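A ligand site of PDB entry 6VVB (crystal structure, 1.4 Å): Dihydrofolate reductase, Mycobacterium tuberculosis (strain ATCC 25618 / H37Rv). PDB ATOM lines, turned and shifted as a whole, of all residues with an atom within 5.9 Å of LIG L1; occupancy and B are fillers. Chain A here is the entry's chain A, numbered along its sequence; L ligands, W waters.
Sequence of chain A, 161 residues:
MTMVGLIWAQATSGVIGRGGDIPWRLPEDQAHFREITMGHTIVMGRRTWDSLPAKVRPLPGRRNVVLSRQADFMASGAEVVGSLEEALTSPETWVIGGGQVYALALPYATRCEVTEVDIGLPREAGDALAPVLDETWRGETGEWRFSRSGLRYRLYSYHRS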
ATOM      1  N   ILE A  22      -2.305 -32.272  19.468  1.00  0.00           N
ATOM      2  CA  ILE A  22      -0.910 -32.690  19.399  1.00  0.00           C
ATOM      3  C   ILE A  22      -0.888 -34.133  18.918  1.00  0.00           C
ATOM      4  O   ILE A  22      -1.605 -34.976  19.482  1.00  0.00           O
ATOM      5  CB  ILE A  22      -0.216 -32.564  20.773  1.00  0.00           C
ATOM      6  CG1 ILE A  22      -0.252 -31.108  21.238  1.00  0.00           C
ATOM      7  CG2 ILE A  22       1.217 -33.087  20.705  1.00  0.00           C
ATOM      8  CD1 ILE A  22       0.199 -30.912  22.671  1.00  0.00           C
ATOM      9  N   GLN A  30       4.349 -35.005  31.849  1.00  0.00           N
ATOM     10  CA  GLN A  30       3.459 -34.111  32.572  1.00  0.00           C
ATOM     11  C   GLN A  30       4.133 -33.577  33.834  1.00  0.00           C
ATOM     12  O   GLN A  30       3.951 -32.405  34.189  1.00  0.00           O
ATOM     13  CB  GLN A  30       2.171 -34.857  32.930  1.00  0.00           C
ATOM     14  CG  GLN A  30       0.967 -33.960  33.156  1.00  0.00           C
ATOM     15  CD  GLN A  30      -0.332 -34.641  32.783  1.00  0.00           C
ATOM     16  OE1 GLN A  30      -1.147 -34.993  33.640  1.00  0.00           O
ATOM     17  NE2 GLN A  30      -0.542 -34.843  31.476  1.00  0.00           N
ATOM     18  N   PHE A  33       6.319 -30.708  32.803  1.00  0.00           N
ATOM     19  CA  PHE A  33       5.498 -29.544  32.480  1.00  0.00           C
ATOM     20  C   PHE A  33       4.997 -28.858  33.743  1.00  0.00           C
ATOM     21  O   PHE A  33       5.025 -27.624  33.844  1.00  0.00           O
ATOM     22  CB  PHE A  33       4.331 -29.956  31.578  1.00  0.00           C
ATOM     23  CG  PHE A  33       3.429 -28.814  31.179  1.00  0.00           C
ATOM     24  CD1 PHE A  33       3.784 -27.971  30.141  1.00  0.00           C
ATOM     25  CD2 PHE A  33       2.213 -28.625  31.802  1.00  0.00           C
ATOM     26  CE1 PHE A  33       2.939 -26.927  29.757  1.00  0.00           C
ATOM     27  CE2 PHE A  33       1.365 -27.591  31.420  1.00  0.00           C
ATOM     28  CZ  PHE A  33       1.728 -26.748  30.394  1.00  0.00           C
ATOM     29  N   ARG A  34       4.562 -29.645  34.731  1.00  0.00           N
ATOM     30  CA  ARG A  34       4.088 -29.075  35.986  1.00  0.00           C
ATOM     31  C   ARG A  34       5.238 -28.454  36.782  1.00  0.00           C
ATOM     32  O   ARG A  34       5.079 -27.359  37.338  1.00  0.00           O
ATOM     33  CB  ARG A  34       3.384 -30.150  36.807  1.00  0.00           C
ATOM     34  CG  ARG A  34       1.994 -30.511  36.307  1.00  0.00           C
ATOM     35  CD  ARG A  34       1.351 -31.598  37.165  1.00  0.00           C
ATOM     36  NE  ARG A  34       1.195 -31.191  38.557  1.00  0.00           N
ATOM     37  CZ  ARG A  34       0.111 -30.599  39.049  1.00  0.00           C
ATOM     38  NH1 ARG A  34      -0.932 -30.341  38.254  1.00  0.00           N
ATOM     39  NH2 ARG A  34       0.053 -30.260  40.330  1.00  0.00           N
ATOM     40  N   THR A  37       6.026 -25.043  35.150  1.00  0.00           N
ATOM     41  CA  THR A  37       5.002 -24.010  35.067  1.00  0.00           C
ATOM     42  C   THR A  37       4.262 -23.732  36.377  1.00  0.00           C
ATOM     43  O   THR A  37       3.692 -22.645  36.513  1.00  0.00           O
ATOM     44  CB  THR A  37       3.956 -24.328  34.000  1.00  0.00           C
ATOM     45  OG1 THR A  37       3.285 -25.555  34.319  1.00  0.00           O
ATOM     46  CG2 THR A  37       4.581 -24.399  32.595  1.00  0.00           C
ATOM     47  N   MET A  38       4.227 -24.675  37.318  1.00  0.00           N
ATOM     48  CA  MET A  38       3.395 -24.520  38.502  1.00  0.00           C
ATOM     49  C   MET A  38       3.722 -23.243  39.274  1.00  0.00           C
ATOM     50  O   MET A  38       4.888 -22.929  39.496  1.00  0.00           O
ATOM     51  CB  MET A  38       3.522 -25.735  39.426  1.00  0.00           C
ATOM     52  CG  MET A  38       2.467 -25.817  40.514  1.00  0.00           C
ATOM     53  SD  MET A  38       0.781 -25.896  39.865  1.00  0.00           S
ATOM     54  CE  MET A  38       0.911 -27.327  38.795  1.00  0.00           C
ATOM     55  N   THR A  48      -4.865 -22.794  21.313  1.00  0.00           N
ATOM     56  CA  THR A  48      -4.384 -23.751  22.303  1.00  0.00           C
ATOM     57  C   THR A  48      -5.331 -23.835  23.498  1.00  0.00           C
ATOM     58  O   THR A  48      -5.631 -24.942  23.972  1.00  0.00           O
ATOM     59  CB  THR A  48      -2.948 -23.390  22.707  1.00  0.00           C
ATOM     60  OG1 THR A  48      -2.081 -23.597  21.585  1.00  0.00           O
ATOM     61  CG2 THR A  48      -2.467 -24.242  23.871  1.00  0.00           C
ATOM     62  N   SER A  51      -8.097 -26.041  22.729  1.00  0.00           N
ATOM     63  CA  SER A  51      -7.696 -27.432  22.630  1.00  0.00           C
ATOM     64  C   SER A  51      -7.600 -28.129  23.981  1.00  0.00           C
ATOM     65  O   SER A  51      -7.516 -29.361  24.019  1.00  0.00           O
ATOM     66  CB  SER A  51      -6.375 -27.517  21.868  1.00  0.00           C
ATOM     67  OG  SER A  51      -5.291 -27.297  22.746  1.00  0.00           O
ATOM     68  N   LEU A  52      -7.638 -27.386  25.076  1.00  0.00           N
ATOM     69  CA  LEU A  52      -7.521 -27.989  26.398  1.00  0.00           C
ATOM     70  C   LEU A  52      -8.815 -28.711  26.759  1.00  0.00           C
ATOM     71  O   LEU A  52      -9.889 -28.128  26.616  1.00  0.00           O
ATOM     72  CB  LEU A  52      -7.255 -26.919  27.447  1.00  0.00           C
ATOM     73  CG  LEU A  52      -5.925 -26.189  27.312  1.00  0.00           C
ATOM     74  CD1 LEU A  52      -5.862 -25.048  28.312  1.00  0.00           C
ATOM     75  CD2 LEU A  52      -4.755 -27.131  27.488  1.00  0.00           C
ATOM     76  N   PRO A  53      -8.752 -29.944  27.234  1.00  0.00           N
ATOM     77  CA  PRO A  53      -9.969 -30.603  27.723  1.00  0.00           C
ATOM     78  C   PRO A  53     -10.542 -29.797  28.890  1.00  0.00           C
ATOM     79  O   PRO A  53      -9.814 -29.185  29.663  1.00  0.00           O
ATOM     80  CB  PRO A  53      -9.489 -31.983  28.173  1.00  0.00           C
ATOM     81  CG  PRO A  53      -8.022 -31.878  28.309  1.00  0.00           C
ATOM     82  CD  PRO A  53      -7.553 -30.794  27.383  1.00  0.00           C
ATOM     83  N   LYS A  55     -11.621 -30.537  31.651  1.00  0.00           N
ATOM     84  CA  LYS A  55     -11.120 -30.914  32.969  1.00  0.00           C
ATOM     85  C   LYS A  55      -9.913 -30.081  33.391  1.00  0.00           C
ATOM     86  O   LYS A  55      -9.701 -29.857  34.588  1.00  0.00           O
ATOM     87  CB  LYS A  55     -10.758 -32.403  32.968  1.00  0.00           C
ATOM     88  CG  LYS A  55      -9.629 -32.741  32.016  1.00  0.00           C
ATOM     89  CD  LYS A  55      -9.615 -34.204  31.591  1.00  0.00           C
ATOM     90  CE  LYS A  55      -8.304 -34.866  31.971  1.00  0.00           C
ATOM     91  NZ  LYS A  55      -7.880 -35.885  30.970  1.00  0.00           N
ATOM     92  N   VAL A  56      -9.117 -29.604  32.437  1.00  0.00           N
ATOM     93  CA  VAL A  56      -7.927 -28.832  32.787  1.00  0.00           C
ATOM     94  C   VAL A  56      -7.966 -27.474  32.099  1.00  0.00           C
ATOM     95  O   VAL A  56      -6.926 -26.943  31.677  1.00  0.00           O
ATOM     96  CB  VAL A  56      -6.631 -29.607  32.446  1.00  0.00           C
ATOM     97  CG1 VAL A  56      -6.407 -30.718  33.460  1.00  0.00           C
ATOM     98  CG2 VAL A  56      -6.710 -30.158  31.049  1.00  0.00           C
ATOM     99  N   LEU A  59      -5.687 -24.523  33.418  1.00  0.00           N
ATOM    100  CA  LEU A  59      -4.719 -25.438  34.017  1.00  0.00           C
ATOM    101  C   LEU A  59      -4.554 -25.056  35.492  1.00  0.00           C
ATOM    102  O   LEU A  59      -4.296 -23.884  35.792  1.00  0.00           O
ATOM    103  CB  LEU A  59      -3.383 -25.356  33.270  1.00  0.00           C
ATOM    104  CG  LEU A  59      -3.390 -26.107  31.937  1.00  0.00           C
ATOM    105  CD1 LEU A  59      -2.341 -25.581  30.962  1.00  0.00           C
ATOM    106  CD2 LEU A  59      -3.189 -27.590  32.185  1.00  0.00           C
ATOM    107  N   PRO A  60      -4.730 -25.993  36.412  1.00  0.00           N
ATOM    108  CA  PRO A  60      -4.795 -25.618  37.831  1.00  0.00           C
ATOM    109  C   PRO A  60      -3.440 -25.206  38.384  1.00  0.00           C
ATOM    110  O   PRO A  60      -2.393 -25.719  37.981  1.00  0.00           O
ATOM    111  CB  PRO A  60      -5.308 -26.891  38.509  1.00  0.00           C
ATOM    112  CG  PRO A  60      -4.905 -28.007  37.579  1.00  0.00           C
ATOM    113  CD  PRO A  60      -5.007 -27.420  36.190  1.00  0.00           C
ATOM    114  N   ARG A  62      -1.895 -22.335  38.162  1.00  0.00           N
ATOM    115  CA  ARG A  62      -1.171 -21.365  37.370  1.00  0.00           C
ATOM    116  C   ARG A  62      -2.117 -20.235  37.008  1.00  0.00           C
ATOM    117  O   ARG A  62      -3.334 -20.423  36.933  1.00  0.00           O
ATOM    118  CB  ARG A  62      -0.616 -22.015  36.099  1.00  0.00           C
ATOM    119  CG  ARG A  62       0.581 -22.935  36.391  1.00  0.00           C
ATOM    120  CD  ARG A  62       0.659 -24.189  35.520  1.00  0.00           C
ATOM    121  NE  ARG A  62      -0.326 -25.186  35.907  1.00  0.00           N
ATOM    122  CZ  ARG A  62      -0.338 -26.456  35.514  1.00  0.00           C
ATOM    123  NH1 ARG A  62       0.600 -26.946  34.705  1.00  0.00           N
ATOM    124  NH2 ARG A  62      -1.308 -27.261  35.943  1.00  0.00           N
ATOM    125  N   ILE A  96       3.115 -21.464  26.596  1.00  0.00           N
ATOM    126  CA  ILE A  96       2.822 -22.889  26.475  1.00  0.00           C
ATOM    127  C   ILE A  96       2.216 -23.236  25.129  1.00  0.00           C
ATOM    128  O   ILE A  96       1.743 -24.366  24.952  1.00  0.00           O
ATOM    129  CB  ILE A  96       1.949 -23.413  27.633  1.00  0.00           C
ATOM    130  CG1 ILE A  96       0.545 -22.796  27.559  1.00  0.00           C
ATOM    131  CG2 ILE A  96       2.639 -23.136  28.960  1.00  0.00           C
ATOM    132  CD1 ILE A  96      -0.518 -23.621  28.318  1.00  0.00           C
ATOM    133  N   GLY A  97       2.218 -22.319  24.166  1.00  0.00           N
ATOM    134  CA  GLY A  97       1.821 -22.614  22.800  1.00  0.00           C
ATOM    135  C   GLY A  97       0.756 -21.662  22.318  1.00  0.00           C
ATOM    136  O   GLY A  97       0.268 -20.797  23.059  1.00  0.00           O
HETATM  137  C1  LIG L   1      -4.893 -33.792  31.288  1.00  0.00           C
HETATM  138  C2  LIG L   1      -0.384 -27.281  25.881  1.00  0.00           C
HETATM  139  C3  LIG L   1      -1.292 -28.074  25.218  1.00  0.00           C
HETATM  140  C4  LIG L   1      -0.216 -27.459  27.238  1.00  0.00           C
HETATM  141  C5  LIG L   1      -2.057 -29.069  25.861  1.00  0.00           C
HETATM  142  C6  LIG L   1      -0.935 -28.414  27.944  1.00  0.00           C
HETATM  143  C7  LIG L   1      -3.519 -30.994  27.386  1.00  0.00           C
HETATM  144  C8  LIG L   1      -2.338 -30.923  32.055  1.00  0.00           C
HETATM  145  C9  LIG L   1      -1.314 -30.254  34.240  1.00  0.00           C
HETATM  146  C10 LIG L   1      -3.917 -32.769  31.869  1.00  0.00           C
HETATM  147  C11 LIG L   1      -1.853 -29.231  27.253  1.00  0.00           C
HETATM  148  C12 LIG L   1      -2.589 -30.200  27.969  1.00  0.00           C
HETATM  149  C13 LIG L   1      -2.240 -31.166  33.413  1.00  0.00           C
HETATM  150  C14 LIG L   1      -3.186 -31.731  31.230  1.00  0.00           C
HETATM  151  C15 LIG L   1      -3.249 -31.420  29.842  1.00  0.00           C
HETATM  152  C16 LIG L   1      -2.991 -32.214  33.956  1.00  0.00           C
HETATM  153  C17 LIG L   1      -3.003 -32.617  35.423  1.00  0.00           C
HETATM  154  F1  LIG L   1      -3.528 -34.010  35.403  1.00  0.00           F
HETATM  155  F2  LIG L   1      -1.661 -32.601  35.985  1.00  0.00           F
HETATM  156  F3  LIG L   1      -3.981 -31.679  36.076  1.00  0.00           F
HETATM  157  N1  LIG L   1      -3.777 -32.949  33.168  1.00  0.00           N
HETATM  158  N2  LIG L   1      -2.470 -30.449  29.323  1.00  0.00           N
HETATM  159  O1  LIG L   1      -0.221 -29.774  33.852  1.00  0.00           O
HETATM  160  O2  LIG L   1      -1.674 -29.976  35.399  1.00  0.00           O
HETATM  161  S1  LIG L   1      -4.218 -32.051  28.561  1.00  0.00           S
HETATM  162  P1  LG2 L   2      -2.109 -20.667  18.753  1.00  0.00           P
HETATM  163  O1  LG2 L   2      -0.736 -20.032  18.690  1.00  0.00           O
HETATM  164  O2  LG2 L   2      -2.388 -21.581  19.877  1.00  0.00           O
HETATM  165  O3  LG2 L   2      -3.320 -19.524  18.751  1.00  0.00           O
HETATM  166  C1  LG2 L   2      -3.427 -18.637  17.615  1.00  0.00           C
HETATM  167  C2  LG2 L   2      -4.432 -17.551  17.985  1.00  0.00           C
HETATM  168  O4  LG2 L   2      -3.685 -16.675  19.088  1.00  0.00           O
HETATM  169  C3  LG2 L   2      -4.689 -16.683  17.033  1.00  0.00           C
HETATM  170  O5  LG2 L   2      -5.748 -17.151  16.114  1.00  0.00           O
HETATM  171  C4  LG2 L   2      -5.167 -15.423  17.818  1.00  0.00           C
HETATM  172  O6  LG2 L   2      -6.352 -15.635  18.438  1.00  0.00           O
HETATM  173  C5  LG2 L   2      -4.111 -15.419  18.920  1.00  0.00           C
HETATM  174  N1  LG2 L   2      -3.007 -14.552  18.526  1.00  0.00           N
HETATM  175  C6  LG2 L   2      -2.045 -15.044  17.743  1.00  0.00           C
HETATM  176  N2  LG2 L   2      -1.191 -14.042  17.527  1.00  0.00           N
HETATM  177  C7  LG2 L   2      -1.642 -12.951  18.180  1.00  0.00           C
HETATM  178  C8  LG2 L   2      -1.173 -11.684  18.292  1.00  0.00           C
HETATM  179  N3  LG2 L   2      -0.077 -10.763  17.894  1.00  0.00           N
HETATM  180  N4  LG2 L   2      -1.857 -10.807  19.020  1.00  0.00           N
HETATM  181  C9  LG2 L   2      -3.007 -11.145  19.635  1.00  0.00           C
HETATM  182  N5  LG2 L   2      -3.476 -12.401  19.531  1.00  0.00           N
HETATM  183  C10 LG2 L   2      -2.776 -13.275  18.785  1.00  0.00           C
HETATM  184  O7  LG2 L   2      -2.485 -21.382  17.322  1.00  0.00           O
HETATM  185  P2  LG2 L   2      -1.588 -22.392  16.429  1.00  0.00           P
HETATM  186  O8  LG2 L   2      -2.553 -22.919  15.387  1.00  0.00           O
HETATM  187  O9  LG2 L   2      -0.356 -21.725  15.889  1.00  0.00           O
HETATM  188  O10 LG2 L   2      -1.142 -23.611  17.432  1.00  0.00           O
HETATM  189  C11 LG2 L   2      -2.168 -24.478  17.895  1.00  0.00           C
HETATM  190  C12 LG2 L   2      -1.697 -25.982  17.627  1.00  0.00           C
HETATM  191  O11 LG2 L   2      -0.443 -26.118  18.500  1.00  0.00           O
HETATM  192  C13 LG2 L   2      -2.534 -26.870  18.041  1.00  0.00           C
HETATM  193  O12 LG2 L   2      -2.432 -28.056  17.179  1.00  0.00           O
HETATM  194  C14 LG2 L   2      -1.992 -27.347  19.516  1.00  0.00           C
HETATM  195  O13 LG2 L   2      -2.513 -28.691  19.842  1.00  0.00           O
HETATM  196  C15 LG2 L   2      -0.713 -27.386  19.311  1.00  0.00           C
HETATM  197  N6  LG2 L   2       0.104 -27.198  20.519  1.00  0.00           N
HETATM  198  C16 LG2 L   2       1.230 -28.011  20.581  1.00  0.00           C
HETATM  199  C17 LG2 L   2       2.106 -27.974  21.753  1.00  0.00           C
HETATM  200  C18 LG2 L   2       3.270 -28.884  21.742  1.00  0.00           C
HETATM  201  O14 LG2 L   2       3.451 -29.782  20.965  1.00  0.00           O
HETATM  202  N7  LG2 L   2       4.185 -28.619  22.773  1.00  0.00           N
HETATM  203  C19 LG2 L   2       1.805 -27.125  23.009  1.00  0.00           C
HETATM  204  C20 LG2 L   2       0.678 -26.092  22.758  1.00  0.00           C
HETATM  205  C21 LG2 L   2      -0.195 -26.209  21.501  1.00  0.00           C
HETATM  206  P3  LG2 L   2      -7.771 -15.026  17.817  1.00  0.00           P
HETATM  207  O15 LG2 L   2      -8.823 -15.343  18.836  1.00  0.00           O
HETATM  208  O16 LG2 L   2      -7.980 -15.775  16.525  1.00  0.00           O
HETATM  209  O17 LG2 L   2      -7.576 -13.556  17.550  1.00  0.00           O
HETATM  210  O   HOH W   1      -3.127 -28.957  22.410  1.00  0.00           O
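NH2 of Arg 62 is in salt-bridge range of O2 of LIG L1. O2 of LIG L1 is in salt-bridge range of NH1 of Arg 34 (3.0 Å). The side-chain amide oxygen of Gln 30 lies close to a nitrogen (N1) of LIG L1 (3.4 Å). The backbone NH (N) of Thr 48 sits at hydrogen-bond distance from an oxygen (O2) of LG2 L2, at 3.1 Å. The side-chain hydroxyl of Thr 48 is in hydrogen-bond range of an oxygen (O2) of LG2 L2, 2.7 Å away.
The backbone carbonyl oxygen (O) of Pro 60 sits at hydrogen-bond distance from the guanidinium group (NH2) of Arg 62, at 2.8 Å. The side-chain hydroxyl (OG1) of Thr 37 sits at hydrogen-bond distance from the guanidinium group (NH1) of Arg 62 (3.0 Å). The backbone carbonyl oxygen (O) of Phe 33 lies within hydrogen-bond range of the side-chain hydroxyl (OG1) of Thr 37, 2.7 Å away.
Phe 33 touches LIG L1. CD2 of Leu 52 touches C11 of LIG L1, 3.6 Å away. Pro 53 touches LIG L1. Lys 55 touches LIG L1. Val 56 touches LIG L1. Leu 59 touches LIG L1. O of Ile 96 touches C2 of LIG L1, at 3.7 Å. Of the 17 residues printed, 10 come within 4 Å of LIG L1. The nearest printed residue that does not touch LIG L1 is Pro 60 (4.1 Å).
Water W1 lies within hydrogen-bond range of O13 of LG2 L2 (2.7 Å) and OG of Ser 51 (2.7 Å).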
